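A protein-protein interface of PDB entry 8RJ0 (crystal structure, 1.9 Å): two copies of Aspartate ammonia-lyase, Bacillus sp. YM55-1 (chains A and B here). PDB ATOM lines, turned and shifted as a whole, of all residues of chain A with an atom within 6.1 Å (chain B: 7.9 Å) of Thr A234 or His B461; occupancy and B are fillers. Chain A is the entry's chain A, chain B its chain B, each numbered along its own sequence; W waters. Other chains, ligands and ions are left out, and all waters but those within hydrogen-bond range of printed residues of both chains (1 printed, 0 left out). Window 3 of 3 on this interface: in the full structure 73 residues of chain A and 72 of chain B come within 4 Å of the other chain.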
ATOM      1  N   GLY A 228      12.516 -14.514  -5.489  1.00  0.00           N
ATOM      2  CA  GLY A 228      13.520 -15.266  -6.231  1.00  0.00           C
ATOM      3  C   GLY A 228      14.117 -16.410  -5.428  1.00  0.00           C
ATOM      4  O   GLY A 228      14.666 -17.362  -5.980  1.00  0.00           O
ATOM      5  N   ALA A 229      13.894 -16.364  -4.122  1.00  0.00           N
ATOM      6  CA  ALA A 229      14.316 -17.408  -3.203  1.00  0.00           C
ATOM      7  C   ALA A 229      13.585 -18.714  -3.457  1.00  0.00           C
ATOM      8  O   ALA A 229      14.113 -19.766  -3.105  1.00  0.00           O
ATOM      9  CB  ALA A 229      14.016 -16.941  -1.770  1.00  0.00           C
ATOM     10  N   THR A 230      12.368 -18.634  -3.987  1.00  0.00           N
ATOM     11  CA  THR A 230      11.457 -19.772  -4.035  1.00  0.00           C
ATOM     12  C   THR A 230      11.373 -20.469  -2.655  1.00  0.00           C
ATOM     13  O   THR A 230      11.164 -19.799  -1.652  1.00  0.00           O
ATOM     14  CB  THR A 230      11.753 -20.710  -5.233  1.00  0.00           C
ATOM     15  OG1 THR A 230      12.901 -21.580  -5.155  1.00  0.00           O
ATOM     16  CG2 THR A 230      11.838 -19.908  -6.535  1.00  0.00           C
ATOM     17  N   ALA A 231      11.547 -21.791  -2.586  1.00  0.00           N
ATOM     18  CA  ALA A 231      11.065 -22.533  -1.442  1.00  0.00           C
ATOM     19  C   ALA A 231      11.927 -22.301  -0.191  1.00  0.00           C
ATOM     20  O   ALA A 231      11.368 -22.214   0.918  1.00  0.00           O
ATOM     21  CB  ALA A 231      11.003 -23.984  -1.789  1.00  0.00           C
ATOM     22  N   VAL A 232      13.239 -22.137  -0.370  1.00  0.00           N
ATOM     23  CA  VAL A 232      14.172 -22.204   0.762  1.00  0.00           C
ATOM     24  C   VAL A 232      15.289 -21.173   0.652  1.00  0.00           C
ATOM     25  O   VAL A 232      16.135 -21.055   1.528  1.00  0.00           O
ATOM     26  CB  VAL A 232      14.633 -23.662   0.616  1.00  0.00           C
ATOM     27  CG1 VAL A 232      16.108 -23.893   0.539  1.00  0.00           C
ATOM     28  CG2 VAL A 232      13.924 -24.584   1.560  1.00  0.00           C
ATOM     29  N   GLY A 233      15.258 -20.371  -0.393  1.00  0.00           N
ATOM     30  CA  GLY A 233      16.292 -19.389  -0.607  1.00  0.00           C
ATOM     31  C   GLY A 233      17.310 -19.783  -1.676  1.00  0.00           C
ATOM     32  O   GLY A 233      18.045 -18.916  -2.085  1.00  0.00           O
ATOM     33  N   THR A 234      17.314 -21.049  -2.123  1.00  0.00           N
ATOM     34  CA  THR A 234      18.234 -21.509  -3.132  1.00  0.00           C
ATOM     35  C   THR A 234      17.850 -20.955  -4.489  1.00  0.00           C
ATOM     36  O   THR A 234      18.685 -20.888  -5.363  1.00  0.00           O
ATOM     37  CB  THR A 234      18.346 -23.029  -3.175  1.00  0.00           C
ATOM     38  OG1 THR A 234      17.031 -23.534  -3.414  1.00  0.00           O
ATOM     39  CG2 THR A 234      19.049 -23.535  -1.924  1.00  0.00           C
ATOM     40  N   GLY A 235      16.601 -20.605  -4.709  1.00  0.00           N
ATOM     41  CA  GLY A 235      16.238 -20.033  -6.007  1.00  0.00           C
ATOM     42  C   GLY A 235      16.026 -21.083  -7.102  1.00  0.00           C
ATOM     43  O   GLY A 235      15.857 -20.760  -8.294  1.00  0.00           O
ATOM     44  N   LEU A 236      15.984 -22.348  -6.666  1.00  0.00           N
ATOM     45  CA  LEU A 236      15.605 -23.439  -7.532  1.00  0.00           C
ATOM     46  C   LEU A 236      14.343 -23.093  -8.307  1.00  0.00           C
ATOM     47  O   LEU A 236      13.356 -22.738  -7.709  1.00  0.00           O
ATOM     48  CB  LEU A 236      15.394 -24.711  -6.728  1.00  0.00           C
ATOM     49  CG  LEU A 236      15.039 -25.936  -7.569  1.00  0.00           C
ATOM     50  CD1 LEU A 236      16.157 -26.108  -8.641  1.00  0.00           C
ATOM     51  CD2 LEU A 236      14.810 -27.156  -6.727  1.00  0.00           C
ATOM     52  N   LEU A 264      19.881 -15.145  -0.143  1.00  0.00           N
ATOM     53  CA  LEU A 264      18.444 -15.361  -0.189  1.00  0.00           C
ATOM     54  C   LEU A 264      18.013 -16.403   0.855  1.00  0.00           C
ATOM     55  O   LEU A 264      16.861 -16.440   1.235  1.00  0.00           O
ATOM     56  CB  LEU A 264      18.088 -15.755  -1.616  1.00  0.00           C
ATOM     57  CG  LEU A 264      18.084 -14.629  -2.664  1.00  0.00           C
ATOM     58  CD1 LEU A 264      17.823 -15.260  -4.036  1.00  0.00           C
ATOM     59  CD2 LEU A 264      17.003 -13.586  -2.433  1.00  0.00           C
ATOM     60  N   VAL A 265      18.915 -17.287   1.281  1.00  0.00           N
ATOM     61  CA  VAL A 265      18.609 -18.292   2.268  1.00  0.00           C
ATOM     62  C   VAL A 265      18.431 -17.597   3.641  1.00  0.00           C
ATOM     63  O   VAL A 265      17.439 -17.804   4.315  1.00  0.00           O
ATOM     64  CB  VAL A 265      19.717 -19.351   2.329  1.00  0.00           C
ATOM     65  CG1 VAL A 265      19.613 -20.089   3.667  1.00  0.00           C
ATOM     66  CG2 VAL A 265      19.717 -20.302   1.130  1.00  0.00           C
ATOM     67  N   THR A 268      15.163 -15.814   3.743  1.00  0.00           N
ATOM     68  CA  THR A 268      13.955 -16.626   3.681  1.00  0.00           C
ATOM     69  C   THR A 268      13.693 -17.192   5.082  1.00  0.00           C
ATOM     70  O   THR A 268      12.565 -17.456   5.443  1.00  0.00           O
ATOM     71  CB  THR A 268      14.092 -17.754   2.658  1.00  0.00           C
ATOM     72  OG1 THR A 268      14.345 -17.136   1.390  1.00  0.00           O
ATOM     73  CG2 THR A 268      12.906 -18.729   2.661  1.00  0.00           C
ATOM     74  N   ILE B 182      26.289 -31.068   1.521  1.00  0.00           N
ATOM     75  CA  ILE B 182      24.944 -31.013   1.001  1.00  0.00           C
ATOM     76  C   ILE B 182      24.028 -31.695   2.008  1.00  0.00           C
ATOM     77  O   ILE B 182      24.419 -32.676   2.638  1.00  0.00           O
ATOM     78  CB  ILE B 182      24.851 -31.642  -0.409  1.00  0.00           C
ATOM     79  CG1 ILE B 182      23.523 -31.351  -1.070  1.00  0.00           C
ATOM     80  CG2 ILE B 182      25.147 -33.153  -0.410  1.00  0.00           C
ATOM     81  CD1 ILE B 182      23.396 -29.965  -1.646  1.00  0.00           C
ATOM     82  N   GLY B 185      17.107 -29.247   2.863  1.00  0.00           N
ATOM     83  CA  GLY B 185      16.374 -28.159   3.495  1.00  0.00           C
ATOM     84  C   GLY B 185      14.984 -28.622   3.927  1.00  0.00           C
ATOM     85  O   GLY B 185      14.399 -29.516   3.310  1.00  0.00           O
ATOM     86  N   VAL B 193      13.898 -29.078  -0.605  1.00  0.00           N
ATOM     87  CA  VAL B 193      14.885 -29.183  -1.657  1.00  0.00           C
ATOM     88  C   VAL B 193      16.268 -29.060  -1.013  1.00  0.00           C
ATOM     89  O   VAL B 193      16.383 -28.593   0.140  1.00  0.00           O
ATOM     90  CB  VAL B 193      14.669 -28.091  -2.731  1.00  0.00           C
ATOM     91  CG1 VAL B 193      13.320 -28.279  -3.443  1.00  0.00           C
ATOM     92  CG2 VAL B 193      14.777 -26.680  -2.168  1.00  0.00           C
ATOM     93  N   PRO B 194      17.344 -29.451  -1.738  1.00  0.00           N
ATOM     94  CA  PRO B 194      18.676 -29.465  -1.171  1.00  0.00           C
ATOM     95  C   PRO B 194      19.157 -28.074  -0.810  1.00  0.00           C
ATOM     96  O   PRO B 194      18.771 -27.066  -1.455  1.00  0.00           O
ATOM     97  CB  PRO B 194      19.571 -30.077  -2.239  1.00  0.00           C
ATOM     98  CG  PRO B 194      18.620 -30.736  -3.190  1.00  0.00           C
ATOM     99  CD  PRO B 194      17.338 -29.923  -3.118  1.00  0.00           C
ATOM    100  N   ILE B 195      20.052 -28.073   0.196  1.00  0.00           N
ATOM    101  CA  ILE B 195      20.685 -26.858   0.646  1.00  0.00           C
ATOM    102  C   ILE B 195      22.071 -27.246   1.169  1.00  0.00           C
ATOM    103  O   ILE B 195      22.332 -28.399   1.484  1.00  0.00           O
ATOM    104  CB  ILE B 195      19.775 -26.166   1.699  1.00  0.00           C
ATOM    105  CG1 ILE B 195      20.224 -24.736   1.969  1.00  0.00           C
ATOM    106  CG2 ILE B 195      19.687 -26.979   3.006  1.00  0.00           C
ATOM    107  CD1 ILE B 195      19.150 -23.836   2.542  1.00  0.00           C
ATOM    108  N   LEU B 196      22.977 -26.278   1.257  1.00  0.00           N
ATOM    109  CA  LEU B 196      24.270 -26.544   1.848  1.00  0.00           C
ATOM    110  C   LEU B 196      24.196 -26.216   3.337  1.00  0.00           C
ATOM    111  O   LEU B 196      23.662 -25.195   3.742  1.00  0.00           O
ATOM    112  CB  LEU B 196      25.315 -25.717   1.109  1.00  0.00           C
ATOM    113  CG  LEU B 196      25.378 -25.983  -0.411  1.00  0.00           C
ATOM    114  CD1 LEU B 196      26.028 -24.874  -1.169  1.00  0.00           C
ATOM    115  CD2 LEU B 196      26.070 -27.329  -0.705  1.00  0.00           C
ATOM    116  N   GLN B 199      25.368 -22.854   3.788  1.00  0.00           N
ATOM    117  CA  GLN B 199      24.372 -21.799   3.610  1.00  0.00           C
ATOM    118  C   GLN B 199      23.547 -21.522   4.897  1.00  0.00           C
ATOM    119  O   GLN B 199      23.157 -20.388   5.140  1.00  0.00           O
ATOM    120  CB  GLN B 199      23.446 -22.141   2.435  1.00  0.00           C
ATOM    121  CG  GLN B 199      24.105 -22.046   1.051  1.00  0.00           C
ATOM    122  CD  GLN B 199      23.236 -22.599  -0.068  1.00  0.00           C
ATOM    123  OE1 GLN B 199      22.674 -23.683   0.019  1.00  0.00           O
ATOM    124  NE2 GLN B 199      23.082 -21.839  -1.125  1.00  0.00           N
ATOM    125  N   ASN B 455      21.021 -32.967 -10.498  1.00  0.00           N
ATOM    126  CA  ASN B 455      22.267 -32.717  -9.816  1.00  0.00           C
ATOM    127  C   ASN B 455      21.981 -31.902  -8.542  1.00  0.00           C
ATOM    128  O   ASN B 455      21.554 -30.755  -8.631  1.00  0.00           O
ATOM    129  CB  ASN B 455      23.219 -32.020 -10.774  1.00  0.00           C
ATOM    130  CG  ASN B 455      24.513 -31.677 -10.083  1.00  0.00           C
ATOM    131  OD1 ASN B 455      24.526 -31.198  -8.937  1.00  0.00           O
ATOM    132  ND2 ASN B 455      25.606 -31.951 -10.749  1.00  0.00           N
ATOM    133  N   PRO B 456      22.184 -32.433  -7.311  1.00  0.00           N
ATOM    134  CA  PRO B 456      21.711 -31.710  -6.114  1.00  0.00           C
ATOM    135  C   PRO B 456      22.485 -30.419  -5.801  1.00  0.00           C
ATOM    136  O   PRO B 456      21.867 -29.404  -5.475  1.00  0.00           O
ATOM    137  CB  PRO B 456      21.777 -32.787  -5.008  1.00  0.00           C
ATOM    138  CG  PRO B 456      22.849 -33.768  -5.479  1.00  0.00           C
ATOM    139  CD  PRO B 456      22.823 -33.738  -7.019  1.00  0.00           C
ATOM    140  N   TYR B 457      23.821 -30.439  -5.983  1.00  0.00           N
ATOM    141  CA  TYR B 457      24.683 -29.279  -5.812  1.00  0.00           C
ATOM    142  C   TYR B 457      24.278 -28.101  -6.710  1.00  0.00           C
ATOM    143  O   TYR B 457      24.349 -26.954  -6.295  1.00  0.00           O
ATOM    144  CB  TYR B 457      26.126 -29.703  -6.083  1.00  0.00           C
ATOM    145  CG  TYR B 457      26.620 -30.728  -5.076  1.00  0.00           C
ATOM    146  CD1 TYR B 457      27.232 -30.337  -3.882  1.00  0.00           C
ATOM    147  CD2 TYR B 457      26.449 -32.083  -5.302  1.00  0.00           C
ATOM    148  CE1 TYR B 457      27.684 -31.266  -2.955  1.00  0.00           C
ATOM    149  CE2 TYR B 457      26.863 -33.019  -4.364  1.00  0.00           C
ATOM    150  CZ  TYR B 457      27.484 -32.616  -3.195  1.00  0.00           C
ATOM    151  OH  TYR B 457      27.846 -33.579  -2.302  1.00  0.00           O
ATOM    152  N   GLU B 458      23.829 -28.367  -7.942  1.00  0.00           N
ATOM    153  CA  GLU B 458      23.441 -27.310  -8.877  1.00  0.00           C
ATOM    154  C   GLU B 458      22.138 -26.620  -8.467  1.00  0.00           C
ATOM    155  O   GLU B 458      21.912 -25.487  -8.852  1.00  0.00           O
ATOM    156  CB  GLU B 458      23.270 -27.952 -10.261  1.00  0.00           C
ATOM    157  CG  GLU B 458      23.730 -27.076 -11.418  1.00  0.00           C
ATOM    158  CD  GLU B 458      25.208 -26.734 -11.319  1.00  0.00           C
ATOM    159  OE1 GLU B 458      26.033 -27.620 -11.004  1.00  0.00           O
ATOM    160  OE2 GLU B 458      25.516 -25.551 -11.545  1.00  0.00           O
ATOM    161  N   MET B 459      21.257 -27.320  -7.726  1.00  0.00           N
ATOM    162  CA  MET B 459      19.977 -26.782  -7.269  1.00  0.00           C
ATOM    163  C   MET B 459      20.080 -25.840  -6.042  1.00  0.00           C
ATOM    164  O   MET B 459      19.094 -25.283  -5.582  1.00  0.00           O
ATOM    165  CB  MET B 459      19.065 -27.924  -6.810  1.00  0.00           C
ATOM    166  CG  MET B 459      18.833 -28.997  -7.812  1.00  0.00           C
ATOM    167  SD  MET B 459      17.754 -30.170  -6.969  1.00  0.00           S
ATOM    168  CE  MET B 459      18.065 -31.433  -8.218  1.00  0.00           C
ATOM    169  N   ILE B 460      21.298 -25.606  -5.581  1.00  0.00           N
ATOM    170  CA  ILE B 460      21.639 -24.877  -4.385  1.00  0.00           C
ATOM    171  C   ILE B 460      21.819 -23.379  -4.667  1.00  0.00           C
ATOM    172  O   ILE B 460      21.944 -22.586  -3.741  1.00  0.00           O
ATOM    173  CB  ILE B 460      22.957 -25.562  -3.985  1.00  0.00           C
ATOM    174  CG1 ILE B 460      22.838 -26.204  -2.702  1.00  0.00           C
ATOM    175  CG2 ILE B 460      24.189 -24.698  -4.146  1.00  0.00           C
ATOM    176  CD1 ILE B 460      21.908 -27.393  -2.725  1.00  0.00           C
ATOM    177  N   HIS B 461      21.934 -23.021  -5.954  1.00  0.00           N
ATOM    178  CA  HIS B 461      22.016 -21.642  -6.426  1.00  0.00           C
ATOM    179  C   HIS B 461      20.929 -21.444  -7.506  1.00  0.00           C
ATOM    180  O   HIS B 461      20.385 -22.411  -8.051  1.00  0.00           O
ATOM    181  CB  HIS B 461      23.443 -21.340  -6.921  1.00  0.00           C
ATOM    182  CG  HIS B 461      23.807 -22.291  -8.026  1.00  0.00           C
ATOM    183  ND1 HIS B 461      23.190 -22.275  -9.267  1.00  0.00           N
ATOM    184  CD2 HIS B 461      24.618 -23.357  -8.037  1.00  0.00           C
ATOM    185  CE1 HIS B 461      23.645 -23.271 -10.010  1.00  0.00           C
ATOM    186  NE2 HIS B 461      24.527 -23.932  -9.293  1.00  0.00           N
ATOM    187  N   PRO B 462      20.465 -20.205  -7.748  1.00  0.00           N
ATOM    188  CA  PRO B 462      19.255 -19.993  -8.543  1.00  0.00           C
ATOM    189  C   PRO B 462      19.375 -20.496  -9.980  1.00  0.00           C
ATOM    190  O   PRO B 462      20.465 -20.619 -10.497  1.00  0.00           O
ATOM    191  CB  PRO B 462      19.031 -18.490  -8.512  1.00  0.00           C
ATOM    192  CG  PRO B 462      19.751 -18.045  -7.261  1.00  0.00           C
ATOM    193  CD  PRO B 462      20.965 -18.976  -7.116  1.00  0.00           C
ATOM    194  N   GLY B 463      18.245 -20.843 -10.575  1.00  0.00           N
ATOM    195  CA  GLY B 463      18.200 -21.279 -11.956  1.00  0.00           C
ATOM    196  C   GLY B 463      17.189 -22.409 -12.126  1.00  0.00           C
ATOM    197  O   GLY B 463      16.783 -23.045 -11.147  1.00  0.00           O
ATOM    198  N   ILE B 464      16.705 -22.519 -13.376  1.00  0.00           N
ATOM    199  CA  ILE B 464      16.128 -23.721 -13.958  1.00  0.00           C
ATOM    200  C   ILE B 464      17.278 -24.671 -14.243  1.00  0.00           C
ATOM    201  O   ILE B 464      18.221 -24.306 -14.950  1.00  0.00           O
ATOM    202  CB  ILE B 464      15.333 -23.339 -15.211  1.00  0.00           C
ATOM    203  CG1 ILE B 464      14.251 -22.290 -14.855  1.00  0.00           C
ATOM    204  CG2 ILE B 464      14.768 -24.572 -15.930  1.00  0.00           C
ATOM    205  CD1 ILE B 464      13.770 -21.425 -16.004  1.00  0.00           C
ATOM    206  N   ALA B 465      17.201 -25.864 -13.642  1.00  0.00           N
ATOM    207  CA  ALA B 465      18.146 -26.945 -13.882  1.00  0.00           C
ATOM    208  C   ALA B 465      18.123 -27.264 -15.383  1.00  0.00           C
ATOM    209  O   ALA B 465      17.052 -27.149 -15.998  1.00  0.00           O
ATOM    210  CB  ALA B 465      17.775 -28.129 -12.996  1.00  0.00           C
HETATM  211  O   HOH W   1      17.358 -26.188  -3.676  1.00  0.00           O
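Water W1 lies within hydrogen-bond range of the side-chain hydroxyl of Thr A234 (2.7 Å), the backbone carbonyl oxygen of Met B459 (2.7 Å) and the backbone carbonyl oxygen of Pro B194 (2.8 Å).
Of chain B, only Pro B194, Met B459, Ile B460, His B461 and Pro B462 come within 4 Å of Thr A234. Of chain A, only Thr A234 comes within 4 Å of His B461. No residue of chain B comes within 4 Å of Gly A233. Printed residues of chain B within 4 Å of Val A265: Ile B195 and Gln B199. Printed residues of chain A within 4 Å of Met B459: Thr A234 (3.4 Å) and Leu A236 (3.9 Å). Gly A228 touches none of the printed residues of chain B. The nearest residue of chain B that does not touch Thr A234 is Val B193 (4.1 Å). The nearest printed residue of chain B that does not touch Gly A235 is His B461 (4.7 Å).
Among the printed residues, pairs that only touch across the chains: Thr A234 with His B461, Gly A235 with Pro B462, Thr A234 with Ile B460, Thr A234 with Pro B194, Val A232 with Ile B195, Leu A236 with Gly B463, Leu A236 with Val B193, Val A265 with Ile B195, Val A265 with Gln B199 and Leu A236 with Met B459.
Printed residues of chain A that touch a printed residue of chain B: Val A232, Thr A234, Gly A235, Leu A236 and Val A265. Hydrophobic or aromatic side chains of chain A within 4 Å of the printed part of chain B: Val A232, Leu A236 and Val A265. Hydrophobic or aromatic side chains of chain B within 4 Å of the printed part of chain A: Val B193, Ile B195, Met B459 and Pro B462. Among the printed residues, no Asp or Glu carboxylate lies within 4 Å of a Lys or Arg side-chain nitrogen of the other chain.
No position is printed for both chains.
The backbone carbonyl oxygen (O) of Ala A229 sits at hydrogen-bond distance from the backbone NH (N) of Gly A235, at 3.1 Å. The side-chain hydroxyl of Thr A230 lies within hydrogen-bond range of the backbone carbonyl oxygen of Leu A236 (2.8 Å). The backbone carbonyl oxygen (O) of Val B193 sits at hydrogen-bond distance from the backbone NH (N) of Gly B185 (2.9 Å). N of Leu B196 lies within hydrogen-bond range of OE1 of Gln B199 (2.9 Å). The side-chain amide nitrogen (NE2) of Gln B199 is in hydrogen-bond range of the backbone carbonyl oxygen (O) of Ile B460, 2.9 Å away. OE2 of Glu B458 is in hydrogen-bond range of NE2 of His B461.
O of Met B459 sits close to OG1 of Thr A234, at 3.5 Å. The backbone carbonyl oxygen of Gly A235 lies within hydrogen-bond range of the backbone NH of Gly B463, at 3.3 Å. N of Pro B462 lies close to O of Thr A234 (3.1 Å).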
